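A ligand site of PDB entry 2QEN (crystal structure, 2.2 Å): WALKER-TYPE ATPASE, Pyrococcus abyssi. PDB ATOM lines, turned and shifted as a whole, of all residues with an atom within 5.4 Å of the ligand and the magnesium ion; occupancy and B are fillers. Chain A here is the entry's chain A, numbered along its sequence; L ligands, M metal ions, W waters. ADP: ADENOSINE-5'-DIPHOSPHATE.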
ATOM      1  N   LEU A   2     -22.334  24.443  11.217  1.00  0.00           N
ATOM      2  CA  LEU A   2     -22.070  23.002  11.181  1.00  0.00           C
ATOM      3  C   LEU A   2     -21.354  22.570   9.906  1.00  0.00           C
ATOM      4  O   LEU A   2     -20.359  21.846   9.953  1.00  0.00           O
ATOM      5  CB  LEU A   2     -23.356  22.183  11.308  1.00  0.00           C
ATOM      6  CG  LEU A   2     -24.003  21.854  12.655  1.00  0.00           C
ATOM      7  CD1 LEU A   2     -25.075  20.785  12.428  1.00  0.00           C
ATOM      8  CD2 LEU A   2     -22.976  21.392  13.700  1.00  0.00           C
ATOM      9  N   ASP A   4     -19.018  23.172   7.819  1.00  0.00           N
ATOM     10  CA  ASP A   4     -17.766  23.919   7.755  1.00  0.00           C
ATOM     11  C   ASP A   4     -16.661  22.915   8.088  1.00  0.00           C
ATOM     12  O   ASP A   4     -16.787  22.173   9.044  1.00  0.00           O
ATOM     13  CB  ASP A   4     -17.778  25.060   8.773  1.00  0.00           C
ATOM     14  CG  ASP A   4     -16.688  26.072   8.527  1.00  0.00           C
ATOM     15  OD1 ASP A   4     -15.500  25.708   8.621  1.00  0.00           O
ATOM     16  OD2 ASP A   4     -17.027  27.238   8.245  1.00  0.00           O
ATOM     17  N   LEU A   5     -15.593  22.915   7.298  1.00  0.00           N
ATOM     18  CA  LEU A   5     -14.518  21.909   7.427  1.00  0.00           C
ATOM     19  C   LEU A   5     -13.428  22.242   8.441  1.00  0.00           C
ATOM     20  O   LEU A   5     -12.670  21.353   8.822  1.00  0.00           O
ATOM     21  CB  LEU A   5     -13.878  21.627   6.064  1.00  0.00           C
ATOM     22  CG  LEU A   5     -14.781  21.096   4.958  1.00  0.00           C
ATOM     23  CD1 LEU A   5     -14.210  21.438   3.589  1.00  0.00           C
ATOM     24  CD2 LEU A   5     -15.009  19.588   5.096  1.00  0.00           C
ATOM     25  N   ARG A   6     -13.325  23.504   8.856  1.00  0.00           N
ATOM     26  CA  ARG A   6     -12.347  23.902   9.885  1.00  0.00           C
ATOM     27  C   ARG A   6     -12.607  23.200  11.227  1.00  0.00           C
ATOM     28  O   ARG A   6     -13.754  22.825  11.502  1.00  0.00           O
ATOM     29  CB  ARG A   6     -12.353  25.430  10.076  1.00  0.00           C
ATOM     30  CG  ARG A   6     -12.164  26.221   8.782  1.00  0.00           C
ATOM     31  CD  ARG A   6     -12.066  27.735   9.020  1.00  0.00           C
ATOM     32  NE  ARG A   6     -13.266  28.284   9.664  1.00  0.00           N
ATOM     33  CZ  ARG A   6     -14.176  29.044   9.060  1.00  0.00           C
ATOM     34  NH1 ARG A   6     -14.065  29.359   7.768  1.00  0.00           N
ATOM     35  NH2 ARG A   6     -15.222  29.489   9.746  1.00  0.00           N
ATOM     36  N   PRO A   7     -11.549  22.983  12.049  1.00  0.00           N
ATOM     37  CA  PRO A   7     -11.729  22.310  13.338  1.00  0.00           C
ATOM     38  C   PRO A   7     -12.711  23.003  14.288  1.00  0.00           C
ATOM     39  O   PRO A   7     -12.709  24.219  14.407  1.00  0.00           O
ATOM     40  CB  PRO A   7     -10.315  22.317  13.941  1.00  0.00           C
ATOM     41  CG  PRO A   7      -9.403  22.456  12.777  1.00  0.00           C
ATOM     42  CD  PRO A   7     -10.139  23.357  11.826  1.00  0.00           C
ATOM     43  N   LYS A   8     -13.546  22.214  14.943  1.00  0.00           N
ATOM     44  CA  LYS A   8     -14.499  22.751  15.910  1.00  0.00           C
ATOM     45  C   LYS A   8     -13.867  22.768  17.309  1.00  0.00           C
ATOM     46  O   LYS A   8     -13.322  21.771  17.777  1.00  0.00           O
ATOM     47  CB  LYS A   8     -15.794  21.959  15.860  1.00  0.00           C
ATOM     48  CG  LYS A   8     -16.468  22.064  14.485  1.00  0.00           C
ATOM     49  CD  LYS A   8     -17.774  21.345  14.376  1.00  0.00           C
ATOM     50  CE  LYS A   8     -18.276  21.348  12.910  1.00  0.00           C
ATOM     51  NZ  LYS A   8     -18.389  22.707  12.264  1.00  0.00           N
ATOM     52  N   ASP A  13     -20.435  25.190  19.035  1.00  0.00           N
ATOM     53  CA  ASP A  13     -20.156  24.708  17.668  1.00  0.00           C
ATOM     54  C   ASP A  13     -20.307  23.189  17.486  1.00  0.00           C
ATOM     55  O   ASP A  13     -20.145  22.663  16.396  1.00  0.00           O
ATOM     56  CB  ASP A  13     -18.757  25.171  17.243  1.00  0.00           C
ATOM     57  CG  ASP A  13     -18.571  26.674  17.407  1.00  0.00           C
ATOM     58  OD1 ASP A  13     -19.587  27.407  17.421  1.00  0.00           O
ATOM     59  OD2 ASP A  13     -17.415  27.130  17.540  1.00  0.00           O
ATOM     60  N   ILE A  14     -20.648  22.507  18.576  1.00  0.00           N
ATOM     61  CA  ILE A  14     -20.769  21.048  18.609  1.00  0.00           C
ATOM     62  C   ILE A  14     -22.250  20.687  18.683  1.00  0.00           C
ATOM     63  O   ILE A  14     -22.944  21.120  19.608  1.00  0.00           O
ATOM     64  CB  ILE A  14     -19.987  20.459  19.852  1.00  0.00           C
ATOM     65  CG1 ILE A  14     -18.456  20.519  19.629  1.00  0.00           C
ATOM     66  CG2 ILE A  14     -20.425  19.020  20.210  1.00  0.00           C
ATOM     67  CD1 ILE A  14     -18.006  19.899  18.323  1.00  0.00           C
ATOM     68  N   PHE A  15     -22.738  19.919  17.701  1.00  0.00           N
ATOM     69  CA  PHE A  15     -24.104  19.382  17.746  1.00  0.00           C
ATOM     70  C   PHE A  15     -24.215  18.297  18.821  1.00  0.00           C
ATOM     71  O   PHE A  15     -23.362  17.419  18.913  1.00  0.00           O
ATOM     72  CB  PHE A  15     -24.533  18.804  16.382  1.00  0.00           C
ATOM     73  CG  PHE A  15     -26.004  18.479  16.290  1.00  0.00           C
ATOM     74  CD1 PHE A  15     -26.928  19.471  15.963  1.00  0.00           C
ATOM     75  CD2 PHE A  15     -26.476  17.176  16.504  1.00  0.00           C
ATOM     76  CE1 PHE A  15     -28.300  19.193  15.884  1.00  0.00           C
ATOM     77  CE2 PHE A  15     -27.842  16.873  16.410  1.00  0.00           C
ATOM     78  CZ  PHE A  15     -28.752  17.884  16.105  1.00  0.00           C
ATOM     79  N   ASP A  16     -25.280  18.383  19.610  1.00  0.00           N
ATOM     80  CA  ASP A  16     -25.530  17.552  20.806  1.00  0.00           C
ATOM     81  C   ASP A  16     -24.336  17.254  21.691  1.00  0.00           C
ATOM     82  O   ASP A  16     -23.691  18.180  22.212  1.00  0.00           O
ATOM     83  CB  ASP A  16     -26.281  16.259  20.470  1.00  0.00           C
ATOM     84  CG  ASP A  16     -27.434  15.987  21.457  1.00  0.00           C
ATOM     85  OD1 ASP A  16     -27.246  16.159  22.696  1.00  0.00           O
ATOM     86  OD2 ASP A  16     -28.545  15.611  20.981  1.00  0.00           O
ATOM     87  N   ARG A  17     -24.051  15.957  21.874  1.00  0.00           N
ATOM     88  CA  ARG A  17     -22.975  15.473  22.773  1.00  0.00           C
ATOM     89  C   ARG A  17     -23.103  15.932  24.230  1.00  0.00           C
ATOM     90  O   ARG A  17     -22.108  16.009  24.960  1.00  0.00           O
ATOM     91  CB  ARG A  17     -21.585  15.773  22.211  1.00  0.00           C
ATOM     92  CG  ARG A  17     -21.239  15.103  20.860  1.00  0.00           C
ATOM     93  CD  ARG A  17     -21.385  13.581  20.894  1.00  0.00           C
ATOM     94  NE  ARG A  17     -20.807  12.931  19.711  1.00  0.00           N
ATOM     95  CZ  ARG A  17     -21.145  11.711  19.274  1.00  0.00           C
ATOM     96  NH1 ARG A  17     -22.075  11.019  19.926  1.00  0.00           N
ATOM     97  NH2 ARG A  17     -20.566  11.197  18.196  1.00  0.00           N
ATOM     98  N   ILE A  39     -14.764   5.096  17.657  1.00  0.00           N
ATOM     99  CA  ILE A  39     -14.344   4.987  16.250  1.00  0.00           C
ATOM    100  C   ILE A  39     -13.714   6.291  15.739  1.00  0.00           C
ATOM    101  O   ILE A  39     -14.063   7.386  16.193  1.00  0.00           O
ATOM    102  CB  ILE A  39     -15.594   4.626  15.375  1.00  0.00           C
ATOM    103  CG1 ILE A  39     -16.292   3.362  15.895  1.00  0.00           C
ATOM    104  CG2 ILE A  39     -15.280   4.452  13.895  1.00  0.00           C
ATOM    105  CD1 ILE A  39     -15.407   2.188  16.115  1.00  0.00           C
ATOM    106  N   ARG A  40     -12.780   6.174  14.805  1.00  0.00           N
ATOM    107  CA  ARG A  40     -12.216   7.341  14.133  1.00  0.00           C
ATOM    108  C   ARG A  40     -13.323   8.146  13.436  1.00  0.00           C
ATOM    109  O   ARG A  40     -14.173   7.564  12.763  1.00  0.00           O
ATOM    110  CB  ARG A  40     -11.166   6.902  13.114  1.00  0.00           C
ATOM    111  CG  ARG A  40     -10.686   8.009  12.179  1.00  0.00           C
ATOM    112  CD  ARG A  40      -9.398   8.649  12.656  1.00  0.00           C
ATOM    113  NE  ARG A  40      -8.251   7.888  12.185  1.00  0.00           N
ATOM    114  CZ  ARG A  40      -7.328   8.332  11.339  1.00  0.00           C
ATOM    115  NH1 ARG A  40      -7.397   9.570  10.849  1.00  0.00           N
ATOM    116  NH2 ARG A  40      -6.323   7.541  10.976  1.00  0.00           N
ATOM    117  N   ARG A  41     -13.300   9.465  13.619  1.00  0.00           N
ATOM    118  CA  ARG A  41     -14.234  10.446  13.005  1.00  0.00           C
ATOM    119  C   ARG A  41     -15.571  10.564  13.722  1.00  0.00           C
ATOM    120  O   ARG A  41     -16.455  11.276  13.253  1.00  0.00           O
ATOM    121  CB  ARG A  41     -14.483  10.169  11.512  1.00  0.00           C
ATOM    122  CG  ARG A  41     -13.300  10.431  10.620  1.00  0.00           C
ATOM    123  CD  ARG A  41     -13.378   9.565   9.389  1.00  0.00           C
ATOM    124  NE  ARG A  41     -12.108   9.615   8.664  1.00  0.00           N
ATOM    125  CZ  ARG A  41     -11.312   8.571   8.445  1.00  0.00           C
ATOM    126  NH1 ARG A  41     -11.636   7.336   8.861  1.00  0.00           N
ATOM    127  NH2 ARG A  41     -10.176   8.778   7.785  1.00  0.00           N
ATOM    128  N   VAL A  42     -15.695   9.865  14.842  1.00  0.00           N
ATOM    129  CA  VAL A  42     -16.932   9.880  15.621  1.00  0.00           C
ATOM    130  C   VAL A  42     -17.143  11.207  16.354  1.00  0.00           C
ATOM    131  O   VAL A  42     -18.258  11.540  16.745  1.00  0.00           O
ATOM    132  CB  VAL A  42     -16.984   8.676  16.607  1.00  0.00           C
ATOM    133  CG1 VAL A  42     -16.123   8.936  17.882  1.00  0.00           C
ATOM    134  CG2 VAL A  42     -18.418   8.315  16.937  1.00  0.00           C
ATOM    135  N   GLY A  43     -16.063  11.951  16.570  1.00  0.00           N
ATOM    136  CA  GLY A  43     -16.119  13.269  17.204  1.00  0.00           C
ATOM    137  C   GLY A  43     -15.394  13.463  18.532  1.00  0.00           C
ATOM    138  O   GLY A  43     -15.737  14.381  19.272  1.00  0.00           O
ATOM    139  N   LYS A  44     -14.386  12.624  18.825  1.00  0.00           N
ATOM    140  CA  LYS A  44     -13.616  12.708  20.089  1.00  0.00           C
ATOM    141  C   LYS A  44     -12.770  13.969  20.232  1.00  0.00           C
ATOM    142  O   LYS A  44     -12.819  14.641  21.279  1.00  0.00           O
ATOM    143  CB  LYS A  44     -12.710  11.471  20.304  1.00  0.00           C
ATOM    144  CG  LYS A  44     -13.390  10.100  20.223  1.00  0.00           C
ATOM    145  CD  LYS A  44     -12.382   8.970  20.473  1.00  0.00           C
ATOM    146  CE  LYS A  44     -11.401   8.769  19.304  1.00  0.00           C
ATOM    147  NZ  LYS A  44     -12.084   8.514  17.951  1.00  0.00           N
ATOM    148  N   SER A  45     -11.958  14.282  19.217  1.00  0.00           N
ATOM    149  CA  SER A  45     -11.150  15.517  19.283  1.00  0.00           C
ATOM    150  C   SER A  45     -12.021  16.763  19.460  1.00  0.00           C
ATOM    151  O   SER A  45     -11.711  17.646  20.269  1.00  0.00           O
ATOM    152  CB  SER A  45     -10.268  15.681  18.051  1.00  0.00           C
ATOM    153  OG  SER A  45      -9.193  14.772  18.108  1.00  0.00           O
ATOM    154  N   SER A  46     -13.107  16.816  18.701  1.00  0.00           N
ATOM    155  CA  SER A  46     -14.032  17.945  18.718  1.00  0.00           C
ATOM    156  C   SER A  46     -14.651  18.143  20.084  1.00  0.00           C
ATOM    157  O   SER A  46     -14.668  19.255  20.592  1.00  0.00           O
ATOM    158  CB  SER A  46     -15.119  17.765  17.665  1.00  0.00           C
ATOM    159  OG  SER A  46     -14.507  17.553  16.399  1.00  0.00           O
ATOM    160  N   LEU A  47     -15.164  17.058  20.681  1.00  0.00           N
ATOM    161  CA  LEU A  47     -15.726  17.078  22.028  1.00  0.00           C
ATOM    162  C   LEU A  47     -14.671  17.513  23.036  1.00  0.00           C
ATOM    163  O   LEU A  47     -14.949  18.355  23.896  1.00  0.00           O
ATOM    164  CB  LEU A  47     -16.283  15.692  22.397  1.00  0.00           C
ATOM    165  CG  LEU A  47     -16.883  15.534  23.795  1.00  0.00           C
ATOM    166  CD1 LEU A  47     -18.224  16.318  23.943  1.00  0.00           C
ATOM    167  CD2 LEU A  47     -17.079  14.053  24.138  1.00  0.00           C
ATOM    168  N   ARG A  49     -11.802  19.330  22.499  1.00  0.00           N
ATOM    169  CA  ARG A  49     -11.480  20.762  22.334  1.00  0.00           C
ATOM    170  C   ARG A  49     -12.532  21.699  22.929  1.00  0.00           C
ATOM    171  O   ARG A  49     -12.179  22.698  23.562  1.00  0.00           O
ATOM    172  CB  ARG A  49     -11.251  21.124  20.855  1.00  0.00           C
ATOM    173  CG  ARG A  49      -9.898  20.680  20.284  1.00  0.00           C
ATOM    174  CD  ARG A  49      -9.621  21.316  18.928  1.00  0.00           C
ATOM    175  NE  ARG A  49     -10.557  20.806  17.917  1.00  0.00           N
ATOM    176  CZ  ARG A  49     -10.350  19.739  17.151  1.00  0.00           C
ATOM    177  NH1 ARG A  49      -9.225  19.049  17.239  1.00  0.00           N
ATOM    178  NH2 ARG A  49     -11.281  19.380  16.294  1.00  0.00           N
ATOM    179  N   ASP A 135      -4.243  13.194  22.851  1.00  0.00           N
ATOM    180  CA  ASP A 135      -5.121  12.758  21.778  1.00  0.00           C
ATOM    181  C   ASP A 135      -4.468  11.639  21.004  1.00  0.00           C
ATOM    182  O   ASP A 135      -3.343  11.800  20.538  1.00  0.00           O
ATOM    183  CB  ASP A 135      -5.465  13.928  20.848  1.00  0.00           C
ATOM    184  CG  ASP A 135      -6.902  13.864  20.322  1.00  0.00           C
ATOM    185  OD1 ASP A 135      -7.613  12.828  20.551  1.00  0.00           O
ATOM    186  OD2 ASP A 135      -7.325  14.864  19.704  1.00  0.00           O
ATOM    187  N   GLU A 136      -5.161  10.509  20.912  1.00  0.00           N
ATOM    188  CA  GLU A 136      -4.643   9.290  20.262  1.00  0.00           C
ATOM    189  C   GLU A 136      -3.380   8.809  20.978  1.00  0.00           C
ATOM    190  O   GLU A 136      -2.315   8.582  20.359  1.00  0.00           O
ATOM    191  CB  GLU A 136      -4.413   9.480  18.749  1.00  0.00           C
ATOM    192  CG  GLU A 136      -5.642   9.944  17.925  1.00  0.00           C
ATOM    193  CD  GLU A 136      -6.761   8.909  17.804  1.00  0.00           C
ATOM    194  OE1 GLU A 136      -6.544   7.711  18.098  1.00  0.00           O
ATOM    195  OE2 GLU A 136      -7.881   9.305  17.387  1.00  0.00           O
ATOM    196  N   SER A 172      -8.811   6.237  19.028  1.00  0.00           N
ATOM    197  CA  SER A 172      -9.667   5.624  18.018  1.00  0.00           C
ATOM    198  C   SER A 172      -9.374   4.129  17.912  1.00  0.00           C
ATOM    199  O   SER A 172     -10.271   3.339  17.601  1.00  0.00           O
ATOM    200  CB  SER A 172      -9.461   6.296  16.663  1.00  0.00           C
ATOM    201  OG  SER A 172      -9.774   7.687  16.725  1.00  0.00           O
ATOM    202  N   PHE A 203     -23.988   8.969  16.099  1.00  0.00           N
ATOM    203  CA  PHE A 203     -25.348   9.446  16.308  1.00  0.00           C
ATOM    204  C   PHE A 203     -26.345   8.365  15.910  1.00  0.00           C
ATOM    205  O   PHE A 203     -26.106   7.621  14.946  1.00  0.00           O
ATOM    206  CB  PHE A 203     -25.638  10.678  15.424  1.00  0.00           C
ATOM    207  CG  PHE A 203     -24.821  11.903  15.762  1.00  0.00           C
ATOM    208  CD1 PHE A 203     -24.420  12.182  17.085  1.00  0.00           C
ATOM    209  CD2 PHE A 203     -24.496  12.819  14.756  1.00  0.00           C
ATOM    210  CE1 PHE A 203     -23.686  13.335  17.380  1.00  0.00           C
ATOM    211  CE2 PHE A 203     -23.767  13.985  15.048  1.00  0.00           C
ATOM    212  CZ  PHE A 203     -23.347  14.237  16.362  1.00  0.00           C
ATOM    213  N   PHE A 211     -29.061  16.592  12.774  1.00  0.00           N
ATOM    214  CA  PHE A 211     -27.753  17.168  12.485  1.00  0.00           C
ATOM    215  C   PHE A 211     -27.762  17.818  11.104  1.00  0.00           C
ATOM    216  O   PHE A 211     -27.470  19.011  10.978  1.00  0.00           O
ATOM    217  CB  PHE A 211     -26.682  16.064  12.575  1.00  0.00           C
ATOM    218  CG  PHE A 211     -25.263  16.558  12.415  1.00  0.00           C
ATOM    219  CD1 PHE A 211     -24.704  16.759  11.140  1.00  0.00           C
ATOM    220  CD2 PHE A 211     -24.462  16.771  13.536  1.00  0.00           C
ATOM    221  CE1 PHE A 211     -23.394  17.206  10.980  1.00  0.00           C
ATOM    222  CE2 PHE A 211     -23.157  17.206  13.395  1.00  0.00           C
ATOM    223  CZ  PHE A 211     -22.617  17.418  12.100  1.00  0.00           C
ATOM    224  N   PRO A 239     -20.278  11.829  12.336  1.00  0.00           N
ATOM    225  CA  PRO A 239     -20.306  13.276  12.112  1.00  0.00           C
ATOM    226  C   PRO A 239     -19.288  13.749  11.072  1.00  0.00           C
ATOM    227  O   PRO A 239     -19.562  14.703  10.373  1.00  0.00           O
ATOM    228  CB  PRO A 239     -19.968  13.851  13.499  1.00  0.00           C
ATOM    229  CG  PRO A 239     -20.358  12.775  14.456  1.00  0.00           C
ATOM    230  CD  PRO A 239     -20.033  11.496  13.753  1.00  0.00           C
ATOM    231  N   GLY A 240     -18.130  13.077  10.981  1.00  0.00           N
ATOM    232  CA  GLY A 240     -17.098  13.440  10.002  1.00  0.00           C
ATOM    233  C   GLY A 240     -17.637  13.410   8.575  1.00  0.00           C
ATOM    234  O   GLY A 240     -17.412  14.337   7.805  1.00  0.00           O
ATOM    235  N   VAL A 243     -20.725  16.055   7.966  1.00  0.00           N
ATOM    236  CA  VAL A 243     -20.201  17.404   7.680  1.00  0.00           C
ATOM    237  C   VAL A 243     -19.630  17.538   6.257  1.00  0.00           C
ATOM    238  O   VAL A 243     -19.906  18.541   5.596  1.00  0.00           O
ATOM    239  CB  VAL A 243     -19.165  17.894   8.742  1.00  0.00           C
ATOM    240  CG1 VAL A 243     -18.475  19.205   8.297  1.00  0.00           C
ATOM    241  CG2 VAL A 243     -19.838  18.122  10.093  1.00  0.00           C
HETATM  242  PB  ADP L   1     -12.195  11.811  16.068  1.00  0.00           P
HETATM  243  O1B ADP L   1     -13.197  11.019  16.876  1.00  0.00           O
HETATM  244  O2B ADP L   1     -11.298  12.645  16.953  1.00  0.00           O
HETATM  245  O3B ADP L   1     -11.435  11.039  15.026  1.00  0.00           O
HETATM  246  PA  ADP L   1     -13.119  14.464  15.148  1.00  0.00           P
HETATM  247  O1A ADP L   1     -13.453  15.101  16.474  1.00  0.00           O
HETATM  248  O2A ADP L   1     -11.940  14.933  14.369  1.00  0.00           O
HETATM  249  O3A ADP L   1     -13.121  12.835  15.251  1.00  0.00           O
HETATM  250  O5' ADP L   1     -14.466  14.639  14.266  1.00  0.00           O
HETATM  251  C5' ADP L   1     -14.501  14.473  12.844  1.00  0.00           C
HETATM  252  C4' ADP L   1     -15.160  15.708  12.232  1.00  0.00           C
HETATM  253  O4' ADP L   1     -16.597  15.627  12.372  1.00  0.00           O
HETATM  254  C3' ADP L   1     -14.808  17.038  12.893  1.00  0.00           C
HETATM  255  O3' ADP L   1     -13.692  17.681  12.272  1.00  0.00           O
HETATM  256  C2' ADP L   1     -16.018  17.877  12.663  1.00  0.00           C
HETATM  257  O2' ADP L   1     -16.013  18.174  11.270  1.00  0.00           O
HETATM  258  C1' ADP L   1     -17.136  16.893  12.760  1.00  0.00           C
HETATM  259  N9  ADP L   1     -17.798  16.706  14.079  1.00  0.00           N
HETATM  260  C8  ADP L   1     -17.507  15.737  14.960  1.00  0.00           C
HETATM  261  N7  ADP L   1     -18.337  15.781  16.032  1.00  0.00           N
HETATM  262  C5  ADP L   1     -19.186  16.810  15.833  1.00  0.00           C
HETATM  263  C6  ADP L   1     -20.319  17.414  16.567  1.00  0.00           C
HETATM  264  N6  ADP L   1     -20.711  16.919  17.761  1.00  0.00           N
HETATM  265  N1  ADP L   1     -20.939  18.484  16.006  1.00  0.00           N
HETATM  266  C2  ADP L   1     -20.548  18.991  14.831  1.00  0.00           C
HETATM  267  N3  ADP L   1     -19.540  18.474  14.097  1.00  0.00           N
HETATM  268  C4  ADP L   1     -18.833  17.403  14.535  1.00  0.00           C
HETATM  269 MG    MG M   1      -9.131  12.792  16.927  1.00  0.00          MG
HETATM  270  O   HOH W   1      -7.068  13.181  16.731  1.00  0.00           O
HETATM  271  O   HOH W   2      -8.728  11.162  15.471  1.00  0.00           O
HETATM  272  O   HOH W   3     -13.494  19.536  14.612  1.00  0.00           O
HETATM  273  O   HOH W   4     -10.749  12.031  12.253  1.00  0.00           O
HETATM  274  O   HOH W   5     -15.382  16.298   8.440  1.00  0.00           O
HETATM  275  O   HOH W   6     -10.953  17.276  14.610  1.00  0.00           O
HETATM  276  O   HOH W   7     -15.456  20.574  10.759  1.00  0.00           O
HETATM  277  O   HOH W   8      -9.362  14.019  15.217  1.00  0.00           O
HETATM  278  O   HOH W   9     -18.495  14.768  18.836  1.00  0.00           O
HETATM  279  O   HOH W  10      -9.031  11.602  18.717  1.00  0.00           O
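The magnesium ion is bound by water W1 (2.1 Å), water W8 (2.1 Å), water W10 (2.2 Å), O2B of the ligand (2.2 Å), water W2 (2.2 Å) and OG of Ser 45 (2.3 Å).
Residues that only touch the magnesium ion: Asp 135 (3.9 Å) and Glu 136 (3.7 Å).
Three residues have an atom within 4 Å of the magnesium ion: Ser 45, Asp 135 and Glu 136.
An oxygen (O1A) of the ligand sits at hydrogen-bond distance from the backbone NH of Ser 45, at 3.2 Å.
N of Ser 46 sits at hydrogen-bond distance from O1A of the ligand (2.8 Å).
The side-chain hydroxyl (OG) of Ser 46 sits at hydrogen-bond distance from an oxygen (O1A) of the ligand, at 2.7 Å.
The backbone NH (N) of Lys 44 is in hydrogen-bond range of an oxygen (O1B) of the ligand (2.8 Å).
An oxygen (O1B) of the ligand lies within salt-bridge range of the side-chain amino group (NZ) of Lys 44 (2.9 Å).
O3B of the ligand lies within hydrogen-bond range of N of Arg 41 (2.8 Å).
A nitrogen (N1) of the ligand lies within hydrogen-bond range of the backbone NH (N) of Phe 15.
O of Phe 15 lies within hydrogen-bond range of N6 of the ligand (2.9 Å).
O1B of the ligand lies within hydrogen-bond range of N of Gly 43, 3.0 Å away.
The backbone NH of Gly 240 lies close to an oxygen (O4') of the ligand.
N of Val 42 lies within hydrogen-bond range of O1B of the ligand, at 3.4 Å.
Residues that only touch the ligand: Leu 2, Lys 8, Ile 14, Arg 17, Ile 39, Arg 40, Phe 211, Pro 239 and Val 243.
Hydrophobic or aromatic side chains within 4 Å of the ligand: Leu 2, Ile 14, Phe 15, Val 42, Phe 211, Pro 239 and Val 243.
Of the 29 residues printed, 17 come within 4 Å of the ligand.
The side-chain hydroxyl (OG) of Ser 45 sits close to the side-chain carboxylate (OD2) of Asp 135.
NZ of Lys 44 lies within hydrogen-bond range of O of Ile 39.
NZ of Lys 44 lies within hydrogen-bond range of OG of Ser 172.
The backbone carbonyl oxygen (O) of Arg 41 sits at hydrogen-bond distance from the backbone NH (N) of Gly 240, at 3.3 Å.
The backbone carbonyl oxygen of Leu 2 is in hydrogen-bond range of the side-chain amino group of Lys 8 (3.2 Å).
The guanidinium group (NE) of Arg 49 lies within hydrogen-bond range of the backbone carbonyl oxygen (O) of Lys 8.
The backbone carbonyl oxygen (O) of Val 42 is in hydrogen-bond range of the guanidinium group (NH2) of Arg 17, at 2.7 Å.
OG of Ser 172 sits at hydrogen-bond distance from OE2 of Glu 136 (2.6 Å).
Water W10 lies within hydrogen-bond range of OD1 of Asp 135 and OE2 of Glu 136.
Water W2 bridges an oxygen (O3B) of the ligand (2.7 Å) and the side-chain carboxylate (OE2) of Glu 136 (2.8 Å).
Water W6 lies within hydrogen-bond range of an oxygen (O2A) of the ligand and the guanidinium group (NH2) of Arg 49.
Water W9 lies within hydrogen-bond range of O of Gly 43, N7 of the ligand and NE of Arg 17.
Water W3 lies within hydrogen-bond range of N of Lys 8 (2.7 Å), NH2 of Arg 49 (2.8 Å), OG of Ser 46 (2.9 Å) and O3' of the ligand (3.0 Å).
Water W5 lies within hydrogen-bond range of the backbone carbonyl oxygen (O) of Gly 240 (2.9 Å) and an oxygen (O2') of the ligand (3.5 Å).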
